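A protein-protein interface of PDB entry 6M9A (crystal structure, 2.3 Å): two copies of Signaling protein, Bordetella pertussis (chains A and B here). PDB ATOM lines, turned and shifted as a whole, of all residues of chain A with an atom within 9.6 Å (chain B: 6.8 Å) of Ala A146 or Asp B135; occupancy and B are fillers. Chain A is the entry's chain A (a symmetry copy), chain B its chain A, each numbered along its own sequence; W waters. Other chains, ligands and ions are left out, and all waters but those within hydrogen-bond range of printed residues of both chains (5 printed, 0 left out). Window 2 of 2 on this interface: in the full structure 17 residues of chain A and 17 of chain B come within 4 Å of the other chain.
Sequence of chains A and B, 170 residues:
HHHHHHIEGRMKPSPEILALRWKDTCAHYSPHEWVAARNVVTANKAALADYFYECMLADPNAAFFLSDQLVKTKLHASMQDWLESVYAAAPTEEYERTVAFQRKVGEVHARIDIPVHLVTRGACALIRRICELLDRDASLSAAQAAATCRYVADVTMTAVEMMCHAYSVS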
ATOM      1  N   TYR A  29       5.188   2.457 -21.978  1.00  0.00           N
ATOM      2  CA  TYR A  29       5.114   2.165 -20.556  1.00  0.00           C
ATOM      3  C   TYR A  29       3.753   1.586 -20.208  1.00  0.00           C
ATOM      4  O   TYR A  29       2.816   1.662 -21.001  1.00  0.00           O
ATOM      5  CB  TYR A  29       5.384   3.429 -19.738  1.00  0.00           C
ATOM      6  CG  TYR A  29       6.658   4.140 -20.133  1.00  0.00           C
ATOM      7  CD1 TYR A  29       7.847   3.899 -19.459  1.00  0.00           C
ATOM      8  CD2 TYR A  29       6.673   5.048 -21.182  1.00  0.00           C
ATOM      9  CE1 TYR A  29       9.015   4.544 -19.818  1.00  0.00           C
ATOM     10  CE2 TYR A  29       7.835   5.697 -21.549  1.00  0.00           C
ATOM     11  CZ  TYR A  29       9.003   5.442 -20.863  1.00  0.00           C
ATOM     12  OH  TYR A  29      10.163   6.086 -21.224  1.00  0.00           O
ATOM     13  N   GLU A  33       2.970   3.179 -14.596  1.00  0.00           N
ATOM     14  CA  GLU A  33       3.825   4.362 -14.672  1.00  0.00           C
ATOM     15  C   GLU A  33       3.000   5.623 -14.875  1.00  0.00           C
ATOM     16  O   GLU A  33       3.301   6.658 -14.274  1.00  0.00           O
ATOM     17  CB  GLU A  33       4.867   4.227 -15.788  1.00  0.00           C
ATOM     18  CG  GLU A  33       6.029   3.317 -15.456  1.00  0.00           C
ATOM     19  CD  GLU A  33       5.727   1.867 -15.766  1.00  0.00           C
ATOM     20  OE1 GLU A  33       5.585   1.529 -16.955  1.00  0.00           O
ATOM     21  OE2 GLU A  33       5.618   1.066 -14.821  1.00  0.00           O
ATOM     22  N   ALA A  36       1.422   6.397 -11.380  1.00  0.00           N
ATOM     23  CA  ALA A  36       2.382   6.850 -10.370  1.00  0.00           C
ATOM     24  C   ALA A  36       2.872   8.263 -10.665  1.00  0.00           C
ATOM     25  O   ALA A  36       2.984   9.095  -9.756  1.00  0.00           O
ATOM     26  CB  ALA A  36       3.560   5.885 -10.281  1.00  0.00           C
ATOM     27  N   CYS A 131      11.013  14.062 -11.029  1.00  0.00           N
ATOM     28  CA  CYS A 131      11.777  12.839 -10.799  1.00  0.00           C
ATOM     29  C   CYS A 131      12.429  12.827  -9.435  1.00  0.00           C
ATOM     30  O   CYS A 131      12.625  11.753  -8.859  1.00  0.00           O
ATOM     31  CB  CYS A 131      12.824  12.651 -11.887  1.00  0.00           C
ATOM     32  SG  CYS A 131      12.005  12.248 -13.419  1.00  0.00           S
ATOM     33  N   LEU A 134       9.704  11.671  -7.239  1.00  0.00           N
ATOM     34  CA  LEU A 134       9.443  10.254  -7.470  1.00  0.00           C
ATOM     35  C   LEU A 134      10.456   9.381  -6.738  1.00  0.00           C
ATOM     36  O   LEU A 134      10.155   8.251  -6.356  1.00  0.00           O
ATOM     37  CB  LEU A 134       9.467   9.941  -8.967  1.00  0.00           C
ATOM     38  CG  LEU A 134       8.154  10.135  -9.726  1.00  0.00           C
ATOM     39  CD1 LEU A 134       8.392  10.083 -11.228  1.00  0.00           C
ATOM     40  CD2 LEU A 134       7.130   9.092  -9.307  1.00  0.00           C
ATOM     41  N   ASP A 135      11.656   9.918  -6.542  1.00  0.00           N
ATOM     42  CA  ASP A 135      12.723   9.200  -5.854  1.00  0.00           C
ATOM     43  C   ASP A 135      12.484   9.143  -4.348  1.00  0.00           C
ATOM     44  O   ASP A 135      12.981   8.249  -3.665  1.00  0.00           O
ATOM     45  CB  ASP A 135      14.077   9.850  -6.146  1.00  0.00           C
ATOM     46  CG  ASP A 135      15.244   8.987  -5.713  1.00  0.00           C
ATOM     47  OD1 ASP A 135      15.259   7.788  -6.060  1.00  0.00           O
ATOM     48  OD2 ASP A 135      16.148   9.507  -5.026  1.00  0.00           O
ATOM     49  N   ASP A 137       9.494   8.841  -3.111  1.00  0.00           N
ATOM     50  CA  ASP A 137       8.287   8.046  -2.922  1.00  0.00           C
ATOM     51  C   ASP A 137       8.633   6.701  -2.295  1.00  0.00           C
ATOM     52  O   ASP A 137       9.246   5.846  -2.934  1.00  0.00           O
ATOM     53  CB  ASP A 137       7.568   7.838  -4.255  1.00  0.00           C
ATOM     54  CG  ASP A 137       6.063   7.742  -4.096  1.00  0.00           C
ATOM     55  OD1 ASP A 137       5.346   8.561  -4.709  1.00  0.00           O
ATOM     56  OD2 ASP A 137       5.597   6.850  -3.359  1.00  0.00           O
ATOM     57  N   LEU A 140       6.694   3.265  -3.601  1.00  0.00           N
ATOM     58  CA  LEU A 140       7.013   2.733  -4.918  1.00  0.00           C
ATOM     59  C   LEU A 140       8.296   1.911  -4.887  1.00  0.00           C
ATOM     60  O   LEU A 140       9.235   2.241  -4.163  1.00  0.00           O
ATOM     61  CB  LEU A 140       7.157   3.874  -5.927  1.00  0.00           C
ATOM     62  CG  LEU A 140       6.271   3.815  -7.173  1.00  0.00           C
ATOM     63  CD1 LEU A 140       4.867   4.305  -6.857  1.00  0.00           C
ATOM     64  CD2 LEU A 140       6.886   4.630  -8.301  1.00  0.00           C
ATOM     65  N   SER A 141       8.334   0.843  -5.678  1.00  0.00           N
ATOM     66  CA  SER A 141       9.510  -0.013  -5.748  1.00  0.00           C
ATOM     67  C   SER A 141      10.611   0.662  -6.568  1.00  0.00           C
ATOM     68  O   SER A 141      10.375   1.609  -7.321  1.00  0.00           O
ATOM     69  CB  SER A 141       9.163  -1.369  -6.364  1.00  0.00           C
ATOM     70  OG  SER A 141       9.022  -1.277  -7.774  1.00  0.00           O
ATOM     71  N   ALA A 142      11.832   0.146  -6.421  1.00  0.00           N
ATOM     72  CA  ALA A 142      12.964   0.680  -7.169  1.00  0.00           C
ATOM     73  C   ALA A 142      12.704   0.642  -8.664  1.00  0.00           C
ATOM     74  O   ALA A 142      12.789   1.667  -9.352  1.00  0.00           O
ATOM     75  CB  ALA A 142      14.231  -0.105  -6.847  1.00  0.00           C
ATOM     76  N   ALA A 143      12.387  -0.539  -9.187  1.00  0.00           N
ATOM     77  CA  ALA A 143      12.198  -0.671 -10.619  1.00  0.00           C
ATOM     78  C   ALA A 143      10.967   0.083 -11.090  1.00  0.00           C
ATOM     79  O   ALA A 143      10.917   0.500 -12.252  1.00  0.00           O
ATOM     80  CB  ALA A 143      12.126  -2.153 -10.997  1.00  0.00           C
ATOM     81  N   GLN A 144       9.989   0.292 -10.211  1.00  0.00           N
ATOM     82  CA  GLN A 144       8.809   1.051 -10.601  1.00  0.00           C
ATOM     83  C   GLN A 144       9.118   2.528 -10.670  1.00  0.00           C
ATOM     84  O   GLN A 144       8.627   3.220 -11.569  1.00  0.00           O
ATOM     85  CB  GLN A 144       7.671   0.806  -9.619  1.00  0.00           C
ATOM     86  CG  GLN A 144       6.414   1.582  -9.928  1.00  0.00           C
ATOM     87  CD  GLN A 144       5.877   1.255 -11.302  1.00  0.00           C
ATOM     88  OE1 GLN A 144       5.996   0.114 -11.766  1.00  0.00           O
ATOM     89  NE2 GLN A 144       5.292   2.244 -11.967  1.00  0.00           N
ATOM     90  N   ALA A 145       9.925   3.026  -9.723  1.00  0.00           N
ATOM     91  CA  ALA A 145      10.283   4.439  -9.726  1.00  0.00           C
ATOM     92  C   ALA A 145      11.162   4.778 -10.918  1.00  0.00           C
ATOM     93  O   ALA A 145      11.067   5.885 -11.462  1.00  0.00           O
ATOM     94  CB  ALA A 145      10.973   4.826  -8.408  1.00  0.00           C
ATOM     95  N   ALA A 146      11.994   3.835 -11.366  1.00  0.00           N
ATOM     96  CA  ALA A 146      12.864   4.105 -12.508  1.00  0.00           C
ATOM     97  C   ALA A 146      12.067   4.173 -13.805  1.00  0.00           C
ATOM     98  O   ALA A 146      12.232   5.105 -14.607  1.00  0.00           O
ATOM     99  CB  ALA A 146      13.958   3.045 -12.595  1.00  0.00           C
ATOM    100  N   ALA A 147      11.199   3.191 -14.032  1.00  0.00           N
ATOM    101  CA  ALA A 147      10.354   3.219 -15.218  1.00  0.00           C
ATOM    102  C   ALA A 147       9.497   4.472 -15.244  1.00  0.00           C
ATOM    103  O   ALA A 147       9.223   5.007 -16.327  1.00  0.00           O
ATOM    104  CB  ALA A 147       9.463   1.967 -15.270  1.00  0.00           C
ATOM    105  N   THR A 148       9.082   4.954 -14.057  1.00  0.00           N
ATOM    106  CA  THR A 148       8.207   6.117 -13.970  1.00  0.00           C
ATOM    107  C   THR A 148       8.965   7.400 -14.306  1.00  0.00           C
ATOM    108  O   THR A 148       8.435   8.275 -15.000  1.00  0.00           O
ATOM    109  CB  THR A 148       7.559   6.202 -12.573  1.00  0.00           C
ATOM    110  OG1 THR A 148       6.881   4.978 -12.287  1.00  0.00           O
ATOM    111  CG2 THR A 148       6.522   7.333 -12.506  1.00  0.00           C
ATOM    112  N   CYS A 149      10.220   7.505 -13.868  1.00  0.00           N
ATOM    113  CA  CYS A 149      11.041   8.640 -14.264  1.00  0.00           C
ATOM    114  C   CYS A 149      11.263   8.676 -15.778  1.00  0.00           C
ATOM    115  O   CYS A 149      11.198   9.746 -16.390  1.00  0.00           O
ATOM    116  CB  CYS A 149      12.367   8.613 -13.504  1.00  0.00           C
ATOM    117  SG  CYS A 149      12.173   8.896 -11.698  1.00  0.00           S
ATOM    118  N   ARG A 150      11.521   7.516 -16.370  1.00  0.00           N
ATOM    119  CA  ARG A 150      11.739   7.431 -17.808  1.00  0.00           C
ATOM    120  C   ARG A 150      10.494   7.898 -18.551  1.00  0.00           C
ATOM    121  O   ARG A 150      10.587   8.551 -19.590  1.00  0.00           O
ATOM    122  CB  ARG A 150      12.099   6.003 -18.216  1.00  0.00           C
ATOM    123  CG  ARG A 150      13.470   5.552 -17.735  1.00  0.00           C
ATOM    124  CD  ARG A 150      14.024   4.437 -18.608  1.00  0.00           C
ATOM    125  NE  ARG A 150      13.162   3.259 -18.602  1.00  0.00           N
ATOM    126  CZ  ARG A 150      13.085   2.395 -17.596  1.00  0.00           C
ATOM    127  NH1 ARG A 150      13.820   2.573 -16.507  1.00  0.00           N
ATOM    128  NH2 ARG A 150      12.272   1.350 -17.678  1.00  0.00           N
ATOM    129  N   TYR A 151       9.328   7.562 -18.010  1.00  0.00           N
ATOM    130  CA  TYR A 151       8.062   7.953 -18.615  1.00  0.00           C
ATOM    131  C   TYR A 151       7.817   9.445 -18.427  1.00  0.00           C
ATOM    132  O   TYR A 151       7.321  10.121 -19.326  1.00  0.00           O
ATOM    133  CB  TYR A 151       6.906   7.154 -18.011  1.00  0.00           C
ATOM    134  CG  TYR A 151       5.555   7.808 -18.199  1.00  0.00           C
ATOM    135  CD1 TYR A 151       4.913   7.776 -19.429  1.00  0.00           C
ATOM    136  CD2 TYR A 151       4.926   8.461 -17.149  1.00  0.00           C
ATOM    137  CE1 TYR A 151       3.680   8.373 -19.606  1.00  0.00           C
ATOM    138  CE2 TYR A 151       3.694   9.061 -17.317  1.00  0.00           C
ATOM    139  CZ  TYR A 151       3.075   9.014 -18.547  1.00  0.00           C
ATOM    140  OH  TYR A 151       1.848   9.609 -18.720  1.00  0.00           O
ATOM    141  N   VAL A 152       8.168   9.952 -17.249  1.00  0.00           N
ATOM    142  CA  VAL A 152       7.990  11.366 -16.947  1.00  0.00           C
ATOM    143  C   VAL A 152       8.710  12.223 -17.978  1.00  0.00           C
ATOM    144  O   VAL A 152       8.118  13.123 -18.567  1.00  0.00           O
ATOM    145  CB  VAL A 152       8.507  11.720 -15.541  1.00  0.00           C
ATOM    146  CG1 VAL A 152       8.806  13.207 -15.448  1.00  0.00           C
ATOM    147  CG2 VAL A 152       7.493  11.311 -14.485  1.00  0.00           C
ATOM    148  N   ALA A 153       9.986  11.931 -18.199  1.00  0.00           N
ATOM    149  CA  ALA A 153      10.786  12.674 -19.165  1.00  0.00           C
ATOM    150  C   ALA A 153      10.218  12.530 -20.574  1.00  0.00           C
ATOM    151  O   ALA A 153      10.176  13.494 -21.335  1.00  0.00           O
ATOM    152  CB  ALA A 153      12.233  12.210 -19.126  1.00  0.00           C
ATOM    153  N   ASP A 154       9.781  11.322 -20.908  1.00  0.00           N
ATOM    154  CA  ASP A 154       9.216  11.041 -22.222  1.00  0.00           C
ATOM    155  C   ASP A 154       7.945  11.843 -22.493  1.00  0.00           C
ATOM    156  O   ASP A 154       7.838  12.522 -23.513  1.00  0.00           O
ATOM    157  CB  ASP A 154       8.924   9.546 -22.367  1.00  0.00           C
ATOM    158  CG  ASP A 154       9.973   8.825 -23.186  1.00  0.00           C
ATOM    159  OD1 ASP A 154      10.854   9.501 -23.757  1.00  0.00           O
ATOM    160  OD2 ASP A 154       9.918   7.581 -23.262  1.00  0.00           O
ATOM    161  N   ILE B 130      19.618   6.274 -23.014  1.00  0.00           N
ATOM    162  CA  ILE B 130      20.697   6.262 -22.033  1.00  0.00           C
ATOM    163  C   ILE B 130      20.166   5.818 -20.675  1.00  0.00           C
ATOM    164  O   ILE B 130      20.804   5.030 -19.971  1.00  0.00           O
ATOM    165  CB  ILE B 130      21.381   7.644 -21.956  1.00  0.00           C
ATOM    166  CG1 ILE B 130      22.234   7.894 -23.213  1.00  0.00           C
ATOM    167  CG2 ILE B 130      22.227   7.742 -20.694  1.00  0.00           C
ATOM    168  CD1 ILE B 130      22.591   9.364 -23.401  1.00  0.00           C
ATOM    169  N   CYS B 131      18.982   6.297 -20.294  1.00  0.00           N
ATOM    170  CA  CYS B 131      18.433   5.916 -18.996  1.00  0.00           C
ATOM    171  C   CYS B 131      17.977   4.475 -18.974  1.00  0.00           C
ATOM    172  O   CYS B 131      18.011   3.838 -17.916  1.00  0.00           O
ATOM    173  CB  CYS B 131      17.287   6.840 -18.608  1.00  0.00           C
ATOM    174  SG  CYS B 131      17.943   8.455 -18.234  1.00  0.00           S
ATOM    175  N   GLU B 132      17.559   3.940 -20.118  1.00  0.00           N
ATOM    176  CA  GLU B 132      17.271   2.517 -20.168  1.00  0.00           C
ATOM    177  C   GLU B 132      18.543   1.698 -19.954  1.00  0.00           C
ATOM    178  O   GLU B 132      18.523   0.690 -19.245  1.00  0.00           O
ATOM    179  CB  GLU B 132      16.604   2.157 -21.495  1.00  0.00           C
ATOM    180  CG  GLU B 132      15.168   2.680 -21.651  1.00  0.00           C
ATOM    181  CD  GLU B 132      14.549   2.294 -22.986  1.00  0.00           C
ATOM    182  OE1 GLU B 132      15.200   1.546 -23.750  1.00  0.00           O
ATOM    183  OE2 GLU B 132      13.412   2.724 -23.274  1.00  0.00           O
ATOM    184  N   LEU B 133      19.641   2.142 -20.557  1.00  0.00           N
ATOM    185  CA  LEU B 133      20.918   1.453 -20.423  1.00  0.00           C
ATOM    186  C   LEU B 133      21.431   1.541 -18.989  1.00  0.00           C
ATOM    187  O   LEU B 133      22.104   0.633 -18.504  1.00  0.00           O
ATOM    188  CB  LEU B 133      21.949   2.039 -21.388  1.00  0.00           C
ATOM    189  CG  LEU B 133      21.747   1.728 -22.872  1.00  0.00           C
ATOM    190  CD1 LEU B 133      22.605   2.639 -23.735  1.00  0.00           C
ATOM    191  CD2 LEU B 133      22.052   0.266 -23.162  1.00  0.00           C
ATOM    192  N   LEU B 134      21.104   2.640 -18.316  1.00  0.00           N
ATOM    193  CA  LEU B 134      21.528   2.853 -16.936  1.00  0.00           C
ATOM    194  C   LEU B 134      20.754   1.954 -15.978  1.00  0.00           C
ATOM    195  O   LEU B 134      21.257   1.576 -14.921  1.00  0.00           O
ATOM    196  CB  LEU B 134      21.349   4.318 -16.538  1.00  0.00           C
ATOM    197  CG  LEU B 134      22.509   5.261 -16.863  1.00  0.00           C
ATOM    198  CD1 LEU B 134      22.082   6.711 -16.695  1.00  0.00           C
ATOM    199  CD2 LEU B 134      23.715   4.950 -15.991  1.00  0.00           C
ATOM    200  N   ASP B 135      19.527   1.612 -16.360  1.00  0.00           N
ATOM    201  CA  ASP B 135      18.672   0.756 -15.546  1.00  0.00           C
ATOM    202  C   ASP B 135      19.116  -0.703 -15.606  1.00  0.00           C
ATOM    203  O   ASP B 135      18.844  -1.482 -14.694  1.00  0.00           O
ATOM    204  CB  ASP B 135      17.214   0.880 -15.993  1.00  0.00           C
ATOM    205  CG  ASP B 135      16.247   0.256 -15.007  1.00  0.00           C
ATOM    206  OD1 ASP B 135      16.354   0.553 -13.799  1.00  0.00           O
ATOM    207  OD2 ASP B 135      15.380  -0.531 -15.440  1.00  0.00           O
ATOM    208  N   ARG B 136      19.801  -1.068 -16.686  1.00  0.00           N
ATOM    209  CA  ARG B 136      20.286  -2.431 -16.866  1.00  0.00           C
ATOM    210  C   ARG B 136      21.673  -2.614 -16.257  1.00  0.00           C
ATOM    211  O   ARG B 136      22.204  -3.724 -16.227  1.00  0.00           O
ATOM    212  CB  ARG B 136      20.311  -2.801 -18.350  1.00  0.00           C
ATOM    213  CG  ARG B 136      18.953  -2.727 -19.031  1.00  0.00           C
ATOM    214  CD  ARG B 136      18.832  -3.762 -20.136  1.00  0.00           C
ATOM    215  NE  ARG B 136      19.377  -3.279 -21.400  1.00  0.00           N
ATOM    216  CZ  ARG B 136      18.827  -2.316 -22.131  1.00  0.00           C
ATOM    217  NH1 ARG B 136      19.391  -1.940 -23.270  1.00  0.00           N
ATOM    218  NH2 ARG B 136      17.711  -1.729 -21.724  1.00  0.00           N
ATOM    219  N   ASP B 137      22.256  -1.521 -15.774  1.00  0.00           N
ATOM    220  CA  ASP B 137      23.577  -1.569 -15.160  1.00  0.00           C
ATOM    221  C   ASP B 137      23.509  -2.288 -13.818  1.00  0.00           C
ATOM    222  O   ASP B 137      22.942  -1.773 -12.854  1.00  0.00           O
ATOM    223  CB  ASP B 137      24.134  -0.157 -14.975  1.00  0.00           C
ATOM    224  CG  ASP B 137      25.644  -0.107 -15.090  1.00  0.00           C
ATOM    225  OD1 ASP B 137      26.153   0.629 -15.961  1.00  0.00           O
ATOM    226  OD2 ASP B 137      26.325  -0.805 -14.310  1.00  0.00           O
ATOM    227  N   ALA B 138      24.094  -3.480 -13.759  1.00  0.00           N
ATOM    228  CA  ALA B 138      24.089  -4.280 -12.538  1.00  0.00           C
ATOM    229  C   ALA B 138      25.226  -3.909 -11.589  1.00  0.00           C
ATOM    230  O   ALA B 138      25.282  -4.392 -10.459  1.00  0.00           O
ATOM    231  CB  ALA B 138      24.143  -5.761 -12.877  1.00  0.00           C
ATOM    232  N   ALA B 145      21.765   4.745  -9.593  1.00  0.00           N
ATOM    233  CA  ALA B 145      21.215   4.750 -10.943  1.00  0.00           C
ATOM    234  C   ALA B 145      20.147   5.820 -11.094  1.00  0.00           C
ATOM    235  O   ALA B 145      20.013   6.412 -12.172  1.00  0.00           O
ATOM    236  CB  ALA B 145      20.660   3.365 -11.308  1.00  0.00           C
ATOM    237  N   ALA B 146      19.403   6.112 -10.025  1.00  0.00           N
ATOM    238  CA  ALA B 146      18.359   7.130 -10.113  1.00  0.00           C
ATOM    239  C   ALA B 146      18.958   8.528 -10.213  1.00  0.00           C
ATOM    240  O   ALA B 146      18.560   9.332 -11.069  1.00  0.00           O
ATOM    241  CB  ALA B 146      17.422   7.024  -8.913  1.00  0.00           C
ATOM    242  N   CYS B 149      20.297   8.972 -13.753  1.00  0.00           N
ATOM    243  CA  CYS B 149      19.280   9.292 -14.744  1.00  0.00           C
ATOM    244  C   CYS B 149      18.856  10.760 -14.665  1.00  0.00           C
ATOM    245  O   CYS B 149      18.688  11.415 -15.699  1.00  0.00           O
ATOM    246  CB  CYS B 149      18.084   8.353 -14.584  1.00  0.00           C
ATOM    247  SG  CYS B 149      18.476   6.604 -14.991  1.00  0.00           S
HETATM  248  O   HOH W   1      14.934   6.054 -14.658  1.00  0.00           O
HETATM  249  O   HOH W   2      12.457  -0.082 -14.510  1.00  0.00           O
HETATM  250  O   HOH W   3      11.927   3.735 -21.105  1.00  0.00           O
HETATM  251  O   HOH W   4      16.353   4.134 -15.738  1.00  0.00           O
HETATM  252  O   HOH W   5      15.770   9.041 -11.644  1.00  0.00           O
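NH1 of Arg A150 lies within salt-bridge range of OD2 of Asp B135 (3.6 Å).
SG of Cys B131 sits close to SG of Cys B149, at 3.8 Å.
O of Arg A150 sits at hydrogen-bond distance from OH of Tyr A29, 3.0 Å away.
Ala B146 touches Asp A135 (CB to OD1, 3.7 Å).
Asp B135 touches Ala A146 (OD1 to CB, 3.7 Å).
Arg A150 touches Cys B131.
Arg A150 touches Glu B132 (CD to CG, 3.7 Å).
Of chain B, only Asp B135 (3.7 Å) comes within 4 Å of Ala A146.
Printed residues of chain A within 4 Å of Glu B132: Arg A150.
Printed residues of chain B within 4 Å of Asp A135: Ala B146 (3.7 Å).
Printed residues of chain A within 4 Å of Ala B146: Asp A135.
The nearest printed residue of chain B that does not touch Arg A150 is Cys B149 (5.8 Å).
Printed residues of chain B that touch a printed residue of chain A: Cys B131, Glu B132, Asp B135 and Ala B146.
Hydrophobic or aromatic side chains of chain B that line the printed part of chain A: Ala B146.
Among the printed residues, 5 pairs touch across the chains.
Among the printed residues, Asp or Glu carboxylates within 4 Å of a Lys or Arg side-chain nitrogen of the other chain: Arg A150 with Asp B135.
Asp A135 touches Ala B146, and with the chains exchanged Ala A146 touches Asp B135.
Water W4 lies within hydrogen-bond range of O of Cys B131 (2.8 Å), NH1 of Arg A150 (3.1 Å) and SG of Cys B149 (3.3 Å).
Water W2 lies within hydrogen-bond range of O of Ala A143, OD2 of Asp B135 and NH2 of Arg A150.
Water W3 lies within hydrogen-bond range of OE2 of Glu B132 (2.8 Å), NE of Arg A150 (2.8 Å) and OH of Tyr A29 (2.9 Å).
Water W5 lies within hydrogen-bond range of O of Ala B146 and SG of Cys A149.
Water W1 bridges the backbone carbonyl oxygen (O) of Ala A146 and the side-chain sulfur (SG) of Cys B149.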
